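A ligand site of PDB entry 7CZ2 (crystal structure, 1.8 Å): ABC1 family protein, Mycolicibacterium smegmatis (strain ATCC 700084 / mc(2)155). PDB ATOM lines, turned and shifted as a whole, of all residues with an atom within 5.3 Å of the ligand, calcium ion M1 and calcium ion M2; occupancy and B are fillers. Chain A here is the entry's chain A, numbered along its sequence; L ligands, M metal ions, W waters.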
ATOM      1  N   ALA A 131      -2.970  22.635  23.591  1.00  0.00           N
ATOM      2  CA  ALA A 131      -2.777  22.686  22.124  1.00  0.00           C
ATOM      3  C   ALA A 131      -1.648  23.630  21.764  1.00  0.00           C
ATOM      4  O   ALA A 131      -1.333  24.585  22.536  1.00  0.00           O
ATOM      5  CB  ALA A 131      -4.078  23.100  21.459  1.00  0.00           C
ATOM      6  N   SER A 132      -1.035  23.404  20.603  1.00  0.00           N
ATOM      7  CA  SER A 132      -0.093  24.382  20.007  1.00  0.00           C
ATOM      8  C   SER A 132      -0.920  25.342  19.172  1.00  0.00           C
ATOM      9  O   SER A 132      -2.011  24.961  18.693  1.00  0.00           O
ATOM     10  CB  SER A 132       1.001  23.730  19.181  1.00  0.00           C
ATOM     11  OG  SER A 132       0.435  22.898  18.200  1.00  0.00           O
ATOM     12  N   ALA A 133      -0.387  26.530  18.983  1.00  0.00           N
ATOM     13  CA  ALA A 133      -0.877  27.563  18.075  1.00  0.00           C
ATOM     14  C   ALA A 133       0.265  27.865  17.096  1.00  0.00           C
ATOM     15  O   ALA A 133       1.411  27.361  17.356  1.00  0.00           O
ATOM     16  CB  ALA A 133      -1.308  28.798  18.844  1.00  0.00           C
ATOM     17  N   SER A 134      -0.035  28.652  16.069  1.00  0.00           N
ATOM     18  CA  SER A 134       0.900  29.038  14.977  1.00  0.00           C
ATOM     19  C   SER A 134       2.228  29.526  15.577  1.00  0.00           C
ATOM     20  O   SER A 134       3.272  29.032  15.164  1.00  0.00           O
ATOM     21  CB  SER A 134       0.261  30.092  14.133  1.00  0.00           C
ATOM     22  OG  SER A 134      -0.869  29.545  13.453  1.00  0.00           O
ATOM     23  N   ILE A 135       2.181  30.498  16.495  1.00  0.00           N
ATOM     24  CA  ILE A 135       3.399  31.068  17.123  1.00  0.00           C
ATOM     25  C   ILE A 135       3.233  31.133  18.655  1.00  0.00           C
ATOM     26  O   ILE A 135       3.747  32.082  19.278  1.00  0.00           O
ATOM     27  CB  ILE A 135       3.709  32.428  16.485  1.00  0.00           C
ATOM     28  CG1 ILE A 135       2.524  33.382  16.540  1.00  0.00           C
ATOM     29  CG2 ILE A 135       4.194  32.233  15.048  1.00  0.00           C
ATOM     30  CD1 ILE A 135       2.878  34.848  16.447  1.00  0.00           C
ATOM     31  N   VAL A 138      -1.625  27.046  23.770  1.00  0.00           N
ATOM     32  CA  VAL A 138      -2.901  27.307  24.475  1.00  0.00           C
ATOM     33  C   VAL A 138      -2.913  26.461  25.741  1.00  0.00           C
ATOM     34  O   VAL A 138      -2.700  25.235  25.698  1.00  0.00           O
ATOM     35  CB  VAL A 138      -4.122  27.047  23.560  1.00  0.00           C
ATOM     36  CG1 VAL A 138      -5.401  27.386  24.265  1.00  0.00           C
ATOM     37  CG2 VAL A 138      -4.041  27.890  22.287  1.00  0.00           C
ATOM     38  N   ALA A 150      -9.615  29.454  27.840  1.00  0.00           N
ATOM     39  CA  ALA A 150      -8.443  29.250  26.959  1.00  0.00           C
ATOM     40  C   ALA A 150      -7.471  30.425  27.130  1.00  0.00           C
ATOM     41  O   ALA A 150      -7.924  31.567  27.080  1.00  0.00           O
ATOM     42  CB  ALA A 150      -8.883  29.197  25.521  1.00  0.00           C
ATOM     43  N   LYS A 152      -4.192  31.785  25.352  1.00  0.00           N
ATOM     44  CA  LYS A 152      -3.272  31.665  24.210  1.00  0.00           C
ATOM     45  C   LYS A 152      -2.079  32.584  24.461  1.00  0.00           C
ATOM     46  O   LYS A 152      -2.287  33.764  24.567  1.00  0.00           O
ATOM     47  CB  LYS A 152      -3.962  31.979  22.887  1.00  0.00           C
ATOM     48  CG  LYS A 152      -3.002  31.772  21.712  1.00  0.00           C
ATOM     49  CD  LYS A 152      -3.630  31.572  20.351  1.00  0.00           C
ATOM     50  CE  LYS A 152      -4.379  32.720  19.749  1.00  0.00           C
ATOM     51  NZ  LYS A 152      -4.840  32.429  18.350  1.00  0.00           N
ATOM     52  N   GLU A 199      -0.415  39.241  13.237  1.00  0.00           N
ATOM     53  CA  GLU A 199      -0.362  38.014  14.030  1.00  0.00           C
ATOM     54  C   GLU A 199       0.446  38.241  15.324  1.00  0.00           C
ATOM     55  O   GLU A 199       0.238  37.520  16.305  1.00  0.00           O
ATOM     56  CB  GLU A 199       0.231  36.872  13.222  1.00  0.00           C
ATOM     57  CG  GLU A 199       0.258  35.565  13.960  1.00  0.00           C
ATOM     58  CD  GLU A 199      -1.105  34.871  14.119  1.00  0.00           C
ATOM     59  OE1 GLU A 199      -2.041  35.215  13.360  1.00  0.00           O
ATOM     60  OE2 GLU A 199      -1.221  34.047  15.062  1.00  0.00           O
ATOM     61  N   TYR A 202      -1.908  40.090  19.239  1.00  0.00           N
ATOM     62  CA  TYR A 202      -3.132  39.331  19.584  1.00  0.00           C
ATOM     63  C   TYR A 202      -4.279  40.267  19.993  1.00  0.00           C
ATOM     64  O   TYR A 202      -5.424  39.787  20.019  1.00  0.00           O
ATOM     65  CB  TYR A 202      -2.901  38.308  20.680  1.00  0.00           C
ATOM     66  CG  TYR A 202      -2.187  37.021  20.385  1.00  0.00           C
ATOM     67  CD1 TYR A 202      -2.003  36.550  19.090  1.00  0.00           C
ATOM     68  CD2 TYR A 202      -1.678  36.248  21.401  1.00  0.00           C
ATOM     69  CE1 TYR A 202      -1.365  35.351  18.831  1.00  0.00           C
ATOM     70  CE2 TYR A 202      -1.037  35.051  21.167  1.00  0.00           C
ATOM     71  CZ  TYR A 202      -0.884  34.580  19.858  1.00  0.00           C
ATOM     72  OH  TYR A 202      -0.277  33.388  19.574  1.00  0.00           O
ATOM     73  N   GLU A 205      -6.697  40.077  16.783  1.00  0.00           N
ATOM     74  CA  GLU A 205      -7.549  38.871  16.760  1.00  0.00           C
ATOM     75  C   GLU A 205      -8.644  39.034  17.829  1.00  0.00           C
ATOM     76  O   GLU A 205      -9.809  38.722  17.560  1.00  0.00           O
ATOM     77  CB  GLU A 205      -6.716  37.593  16.826  1.00  0.00           C
ATOM     78  CG  GLU A 205      -6.741  36.761  18.076  1.00  0.00           C
ATOM     79  CD  GLU A 205      -6.248  35.340  17.819  1.00  0.00           C
ATOM     80  OE1 GLU A 205      -5.165  35.187  17.187  1.00  0.00           O
ATOM     81  OE2 GLU A 205      -6.988  34.369  18.130  1.00  0.00           O
ATOM     82  N   PRO A 225     -16.697  32.275  21.594  1.00  0.00           N
ATOM     83  CA  PRO A 225     -16.309  32.538  22.977  1.00  0.00           C
ATOM     84  C   PRO A 225     -16.121  34.020  23.218  1.00  0.00           C
ATOM     85  O   PRO A 225     -15.617  34.747  22.349  1.00  0.00           O
ATOM     86  CB  PRO A 225     -14.962  31.884  23.157  1.00  0.00           C
ATOM     87  CG  PRO A 225     -14.875  30.921  22.016  1.00  0.00           C
ATOM     88  CD  PRO A 225     -15.669  31.524  20.883  1.00  0.00           C
ATOM     89  N   SER A 237      -9.948  33.824  26.621  1.00  0.00           N
ATOM     90  CA  SER A 237     -11.344  33.726  26.148  1.00  0.00           C
ATOM     91  C   SER A 237     -12.010  32.550  26.881  1.00  0.00           C
ATOM     92  O   SER A 237     -11.329  31.642  27.429  1.00  0.00           O
ATOM     93  CB  SER A 237     -11.354  33.539  24.642  1.00  0.00           C
ATOM     94  OG  SER A 237     -10.635  32.384  24.310  1.00  0.00           O
ATOM     95  N   GLU A 238     -13.314  32.484  26.767  1.00  0.00           N
ATOM     96  CA  GLU A 238     -14.133  31.386  27.299  1.00  0.00           C
ATOM     97  C   GLU A 238     -13.763  30.065  26.627  1.00  0.00           C
ATOM     98  O   GLU A 238     -13.601  30.060  25.430  1.00  0.00           O
ATOM     99  CB  GLU A 238     -15.594  31.667  26.978  1.00  0.00           C
ATOM    100  CG  GLU A 238     -16.125  32.763  27.892  1.00  0.00           C
ATOM    101  CD  GLU A 238     -17.558  33.132  27.638  1.00  0.00           C
ATOM    102  OE1 GLU A 238     -18.048  32.940  26.476  1.00  0.00           O
ATOM    103  OE2 GLU A 238     -18.161  33.661  28.635  1.00  0.00           O
ATOM    104  N   TRP A 239     -13.551  29.017  27.394  1.00  0.00           N
ATOM    105  CA  TRP A 239     -13.253  27.671  26.867  1.00  0.00           C
ATOM    106  C   TRP A 239     -14.465  27.199  26.097  1.00  0.00           C
ATOM    107  O   TRP A 239     -15.573  27.347  26.617  1.00  0.00           O
ATOM    108  CB  TRP A 239     -12.946  26.705  28.001  1.00  0.00           C
ATOM    109  CG  TRP A 239     -12.557  25.372  27.513  1.00  0.00           C
ATOM    110  CD1 TRP A 239     -13.369  24.264  27.465  1.00  0.00           C
ATOM    111  CD2 TRP A 239     -11.308  24.991  26.916  1.00  0.00           C
ATOM    112  NE1 TRP A 239     -12.693  23.219  26.915  1.00  0.00           N
ATOM    113  CE2 TRP A 239     -11.434  23.629  26.564  1.00  0.00           C
ATOM    114  CE3 TRP A 239     -10.073  25.636  26.712  1.00  0.00           C
ATOM    115  CZ2 TRP A 239     -10.399  22.912  25.966  1.00  0.00           C
ATOM    116  CZ3 TRP A 239      -9.063  24.947  26.083  1.00  0.00           C
ATOM    117  CH2 TRP A 239      -9.201  23.588  25.781  1.00  0.00           C
ATOM    118  N   MET A 240     -14.264  26.671  24.923  1.00  0.00           N
ATOM    119  CA  MET A 240     -15.348  26.134  24.069  1.00  0.00           C
ATOM    120  C   MET A 240     -15.276  24.617  24.200  1.00  0.00           C
ATOM    121  O   MET A 240     -14.281  24.042  23.727  1.00  0.00           O
ATOM    122  CB  MET A 240     -15.112  26.568  22.619  1.00  0.00           C
ATOM    123  CG  MET A 240     -16.216  26.084  21.674  1.00  0.00           C
ATOM    124  SD  MET A 240     -17.775  26.878  22.024  1.00  0.00           S
ATOM    125  CE  MET A 240     -17.391  28.599  21.804  1.00  0.00           C
ATOM    126  N   ASP A 281     -10.464  31.632   7.928  1.00  0.00           N
ATOM    127  CA  ASP A 281      -9.602  30.435   8.073  1.00  0.00           C
ATOM    128  C   ASP A 281     -10.473  29.209   8.321  1.00  0.00           C
ATOM    129  O   ASP A 281     -10.780  28.863   9.511  1.00  0.00           O
ATOM    130  CB  ASP A 281      -8.586  30.662   9.197  1.00  0.00           C
ATOM    131  CG  ASP A 281      -7.555  29.566   9.322  1.00  0.00           C
ATOM    132  OD1 ASP A 281      -7.528  28.663   8.473  1.00  0.00           O
ATOM    133  OD2 ASP A 281      -6.776  29.603  10.235  1.00  0.00           O
ATOM    134  N   GLY A 285      -9.151  22.929  12.919  1.00  0.00           N
ATOM    135  CA  GLY A 285      -8.738  23.255  14.292  1.00  0.00           C
ATOM    136  C   GLY A 285      -9.535  24.436  14.812  1.00  0.00           C
ATOM    137  O   GLY A 285      -9.448  24.670  16.049  1.00  0.00           O
ATOM    138  N   ASN A 286     -10.270  25.160  13.983  1.00  0.00           N
ATOM    139  CA  ASN A 286     -10.990  26.425  14.379  1.00  0.00           C
ATOM    140  C   ASN A 286     -12.439  26.148  14.760  1.00  0.00           C
ATOM    141  O   ASN A 286     -13.176  27.124  15.032  1.00  0.00           O
ATOM    142  CB  ASN A 286     -10.911  27.477  13.301  1.00  0.00           C
ATOM    143  CG  ASN A 286      -9.484  27.933  13.094  1.00  0.00           C
ATOM    144  OD1 ASN A 286      -8.631  27.652  13.924  1.00  0.00           O
ATOM    145  ND2 ASN A 286      -9.180  28.552  11.964  1.00  0.00           N
ATOM    146  N   MET A 288     -15.619  23.390  16.401  1.00  0.00           N
ATOM    147  CA  MET A 288     -16.100  22.244  17.117  1.00  0.00           C
ATOM    148  C   MET A 288     -17.619  22.066  17.196  1.00  0.00           C
ATOM    149  O   MET A 288     -18.328  22.958  16.993  1.00  0.00           O
ATOM    150  CB  MET A 288     -15.541  22.275  18.477  1.00  0.00           C
ATOM    151  CG  MET A 288     -16.156  23.244  19.350  1.00  0.00           C
ATOM    152  SD  MET A 288     -14.809  23.484  20.474  1.00  0.00           S
ATOM    153  CE  MET A 288     -13.844  24.488  19.323  1.00  0.00           C
ATOM    154  N   ILE A 298     -13.688  29.436  16.705  1.00  0.00           N
ATOM    155  CA  ILE A 298     -12.545  30.110  17.368  1.00  0.00           C
ATOM    156  C   ILE A 298     -11.582  30.601  16.289  1.00  0.00           C
ATOM    157  O   ILE A 298     -11.785  30.286  15.077  1.00  0.00           O
ATOM    158  CB  ILE A 298     -11.883  29.185  18.388  1.00  0.00           C
ATOM    159  CG1 ILE A 298     -11.278  27.958  17.719  1.00  0.00           C
ATOM    160  CG2 ILE A 298     -12.820  28.822  19.508  1.00  0.00           C
ATOM    161  CD1 ILE A 298     -10.414  27.106  18.599  1.00  0.00           C
ATOM    162  N   ASP A 299     -10.543  31.301  16.737  1.00  0.00           N
ATOM    163  CA  ASP A 299      -9.408  31.809  15.905  1.00  0.00           C
ATOM    164  C   ASP A 299      -9.895  32.896  14.952  1.00  0.00           C
ATOM    165  O   ASP A 299     -10.343  32.571  13.837  1.00  0.00           O
ATOM    166  CB  ASP A 299      -8.726  30.647  15.167  1.00  0.00           C
ATOM    167  CG  ASP A 299      -7.533  31.119  14.351  1.00  0.00           C
ATOM    168  OD1 ASP A 299      -7.245  32.347  14.405  1.00  0.00           O
ATOM    169  OD2 ASP A 299      -6.926  30.289  13.694  1.00  0.00           O
ATOM    170  N   GLY A 301      -7.852  35.449  13.987  1.00  0.00           N
ATOM    171  CA  GLY A 301      -6.624  36.080  13.497  1.00  0.00           C
ATOM    172  C   GLY A 301      -6.711  36.491  12.025  1.00  0.00           C
ATOM    173  O   GLY A 301      -5.983  37.459  11.658  1.00  0.00           O
ATOM    174  N   ALA A 302      -7.566  35.839  11.226  1.00  0.00           N
ATOM    175  CA  ALA A 302      -7.550  36.000   9.753  1.00  0.00           C
ATOM    176  C   ALA A 302      -8.891  36.339   9.124  1.00  0.00           C
ATOM    177  O   ALA A 302      -9.111  35.811   8.028  1.00  0.00           O
ATOM    178  CB  ALA A 302      -7.026  34.750   9.143  1.00  0.00           C
HETATM  179  P1  LIG L   1      -3.694  29.848  16.059  1.00  0.00           P
HETATM  180  O1  LIG L   1      -2.683  28.822  15.760  1.00  0.00           O
HETATM  181  O2  LIG L   1      -4.731  30.089  14.938  1.00  0.00           O
HETATM  182  O3  LIG L   1      -3.062  31.184  16.432  1.00  0.00           O
HETATM  183  P2  LIG L   1      -5.887  28.915  17.719  1.00  0.00           P
HETATM  184  O4  LIG L   1      -6.555  28.175  16.571  1.00  0.00           O
HETATM  185  O5  LIG L   1      -6.654  30.125  18.130  1.00  0.00           O
HETATM  186  O6  LIG L   1      -4.357  29.227  17.372  1.00  0.00           O
HETATM  187  O7  LIG L   1      -5.677  27.992  18.964  1.00  0.00           O
HETATM  188  C1  LIG L   1      -5.011  26.721  18.817  1.00  0.00           C
HETATM  189  C2  LIG L   1      -5.871  25.593  19.305  1.00  0.00           C
HETATM  190  O8  LIG L   1      -6.149  25.734  20.735  1.00  0.00           O
HETATM  191  C3  LIG L   1      -7.245  25.416  18.670  1.00  0.00           C
HETATM  192  O9  LIG L   1      -7.122  24.735  17.409  1.00  0.00           O
HETATM  193  C4  LIG L   1      -7.946  24.584  19.743  1.00  0.00           C
HETATM  194  O10 LIG L   1      -7.532  23.234  19.713  1.00  0.00           O
HETATM  195  C5  LIG L   1      -7.441  25.277  21.009  1.00  0.00           C
HETATM  196  N1  LIG L   1      -8.241  26.419  21.453  1.00  0.00           N
HETATM  197  C6  LIG L   1      -8.040  27.754  21.219  1.00  0.00           C
HETATM  198  N2  LIG L   1      -8.965  28.535  21.744  1.00  0.00           N
HETATM  199  C7  LIG L   1      -9.858  27.661  22.334  1.00  0.00           C
HETATM  200  C8  LIG L   1     -11.025  27.887  23.090  1.00  0.00           C
HETATM  201  N3  LIG L   1     -11.613  29.095  23.277  1.00  0.00           N
HETATM  202  N4  LIG L   1     -11.629  26.780  23.566  1.00  0.00           N
HETATM  203  C9  LIG L   1     -11.100  25.564  23.324  1.00  0.00           C
HETATM  204  N5  LIG L   1     -10.003  25.245  22.646  1.00  0.00           N
HETATM  205  C10 LIG L   1      -9.396  26.353  22.194  1.00  0.00           C
HETATM  206 CA    CA M   1      -5.006  31.852  13.484  1.00  0.00          CA
HETATM  207 CA    CA M   2      -6.253  28.165  14.289  1.00  0.00          CA
HETATM  208  O   HOH W   1      -4.388  33.541  15.140  1.00  0.00           O
HETATM  209  O   HOH W   2      -4.360  33.913  12.313  1.00  0.00           O
HETATM  210  O   HOH W   3      -5.949  27.538  11.986  1.00  0.00           O
HETATM  211  O   HOH W   4      -0.626  32.265  17.116  1.00  0.00           O
HETATM  212  O   HOH W   5      -6.355  32.193  11.422  1.00  0.00           O
HETATM  213  O   HOH W   6      -6.144  25.583  14.796  1.00  0.00           O
HETATM  214  O   HOH W   7      -9.756  22.558  22.193  1.00  0.00           O
HETATM  215  O   HOH W   8      -5.550  22.320  17.485  1.00  0.00           O
HETATM  216  O   HOH W   9      -4.081  27.166  14.351  1.00  0.00           O
HETATM  217  O   HOH W  10      -2.426  31.777  13.409  1.00  0.00           O
HETATM  218  O   HOH W  11     -11.592  31.590  21.885  1.00  0.00           O
HETATM  219  O   HOH W  12      -9.792  21.589  19.307  1.00  0.00           O
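Water W10 lies within hydrogen-bond range of the side-chain hydroxyl (OG) of Ser 134 (2.7 Å), the side-chain carboxylate (OE2) of Glu 199 (3.1 Å) and an oxygen (O3) of the ligand (3.1 Å). Water W1 lies within hydrogen-bond range of the side-chain carboxylate (OE1) of Glu 205 (2.7 Å), an oxygen (O3) of the ligand (3.0 Å), the side-chain carboxylate (OE2) of Glu 199 (3.2 Å) and the side-chain amino group (NZ) of Lys 152 (3.4 Å). Water W3 bridges the side-chain carboxylate of Asp 281 and the side-chain amide nitrogen of Asn 286. Water W4 lies within hydrogen-bond range of OH of Tyr 202 (2.7 Å), O3 of the ligand (2.8 Å), OE2 of Glu 199 (2.8 Å) and N of Ile 135 (3.4 Å). Water W11 bridges the side-chain hydroxyl of Ser 237 (2.7 Å) and a nitrogen (N3) of the ligand (2.9 Å).
Calcium ion M2 is bound by an oxygen (O4) of the ligand, the side-chain carboxylate (OD2) of Asp 299, water W9, water W3, the side-chain amide oxygen (OD1) of Asn 286, an oxygen (O2) of the ligand and water W6. Calcium ion M2 has seven donor atoms within binding distance.
Within 4 Å of calcium ion M2: Asn 286 and Asp 299. Along chain A the residues within 4 Å of calcium ion M2 span positions 286 to 299.
The backbone NH (N) of Ala 150 sits at hydrogen-bond distance from the backbone carbonyl oxygen (O) of Ser 237 (2.8 Å). The backbone carbonyl oxygen (O) of Asn 286 is in hydrogen-bond range of the backbone NH (N) of Ile 298 (2.9 Å). The side-chain carboxylate (OE2) of Glu 205 is in salt-bridge range of the side-chain amino group (NZ) of Lys 152 (2.9 Å). OD1 of Asp 299 sits close to N of Gly 301, 3.2 Å away. N of Val 138 lies within hydrogen-bond range of O of Ala 131, 2.8 Å away. O of Asp 281 sits at hydrogen-bond distance from ND2 of Asn 286 (2.9 Å).
One residue has an atom within 4 Å of calcium ion M1: Asp 299.
CB of Ala 131 touches O8 of the ligand (3.4 Å). Ser 132 touches the ligand. Ala 133 touches the ligand. Val 138 touches the ligand (CG2 to O8, 3.4 Å). CB of Ala 150 touches C8 of the ligand, at 3.5 Å. Glu 199 touches the ligand. CG of Pro 225 touches N3 of the ligand, at 3.9 Å. Ser 237 touches the ligand (OG to N3, 3.6 Å). Trp 239 touches the ligand (CZ3 to C9, 3.5 Å). Ile 298 touches the ligand (CD1 to C3, 3.6 Å).
Calcium ion M1 is bound by O2 of the ligand (2.3 Å), water W1 (2.4 Å), water W2 (2.5 Å), OD1 of Asp 299 (2.5 Å), OD2 of Asp 299 (2.5 Å), water W5 (2.5 Å) and water W10 (2.6 Å). Calcium ion M1 has seven donor atoms within binding distance.
O of Gly 285 is in hydrogen-bond range of O9 of the ligand (2.7 Å). N4 of the ligand is in hydrogen-bond range of N of Met 240, at 3.0 Å. The side-chain hydroxyl (OG) of Ser 134 is in hydrogen-bond range of an oxygen (O1) of the ligand (3.0 Å). The backbone NH (N) of Ser 134 is in hydrogen-bond range of an oxygen (O1) of the ligand (2.7 Å). The backbone carbonyl oxygen (O) of Glu 238 is in hydrogen-bond range of a nitrogen (N3) of the ligand (3.1 Å). The side-chain amino group (NZ) of Lys 152 lies within salt-bridge range of an oxygen (O3) of the ligand (2.9 Å).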
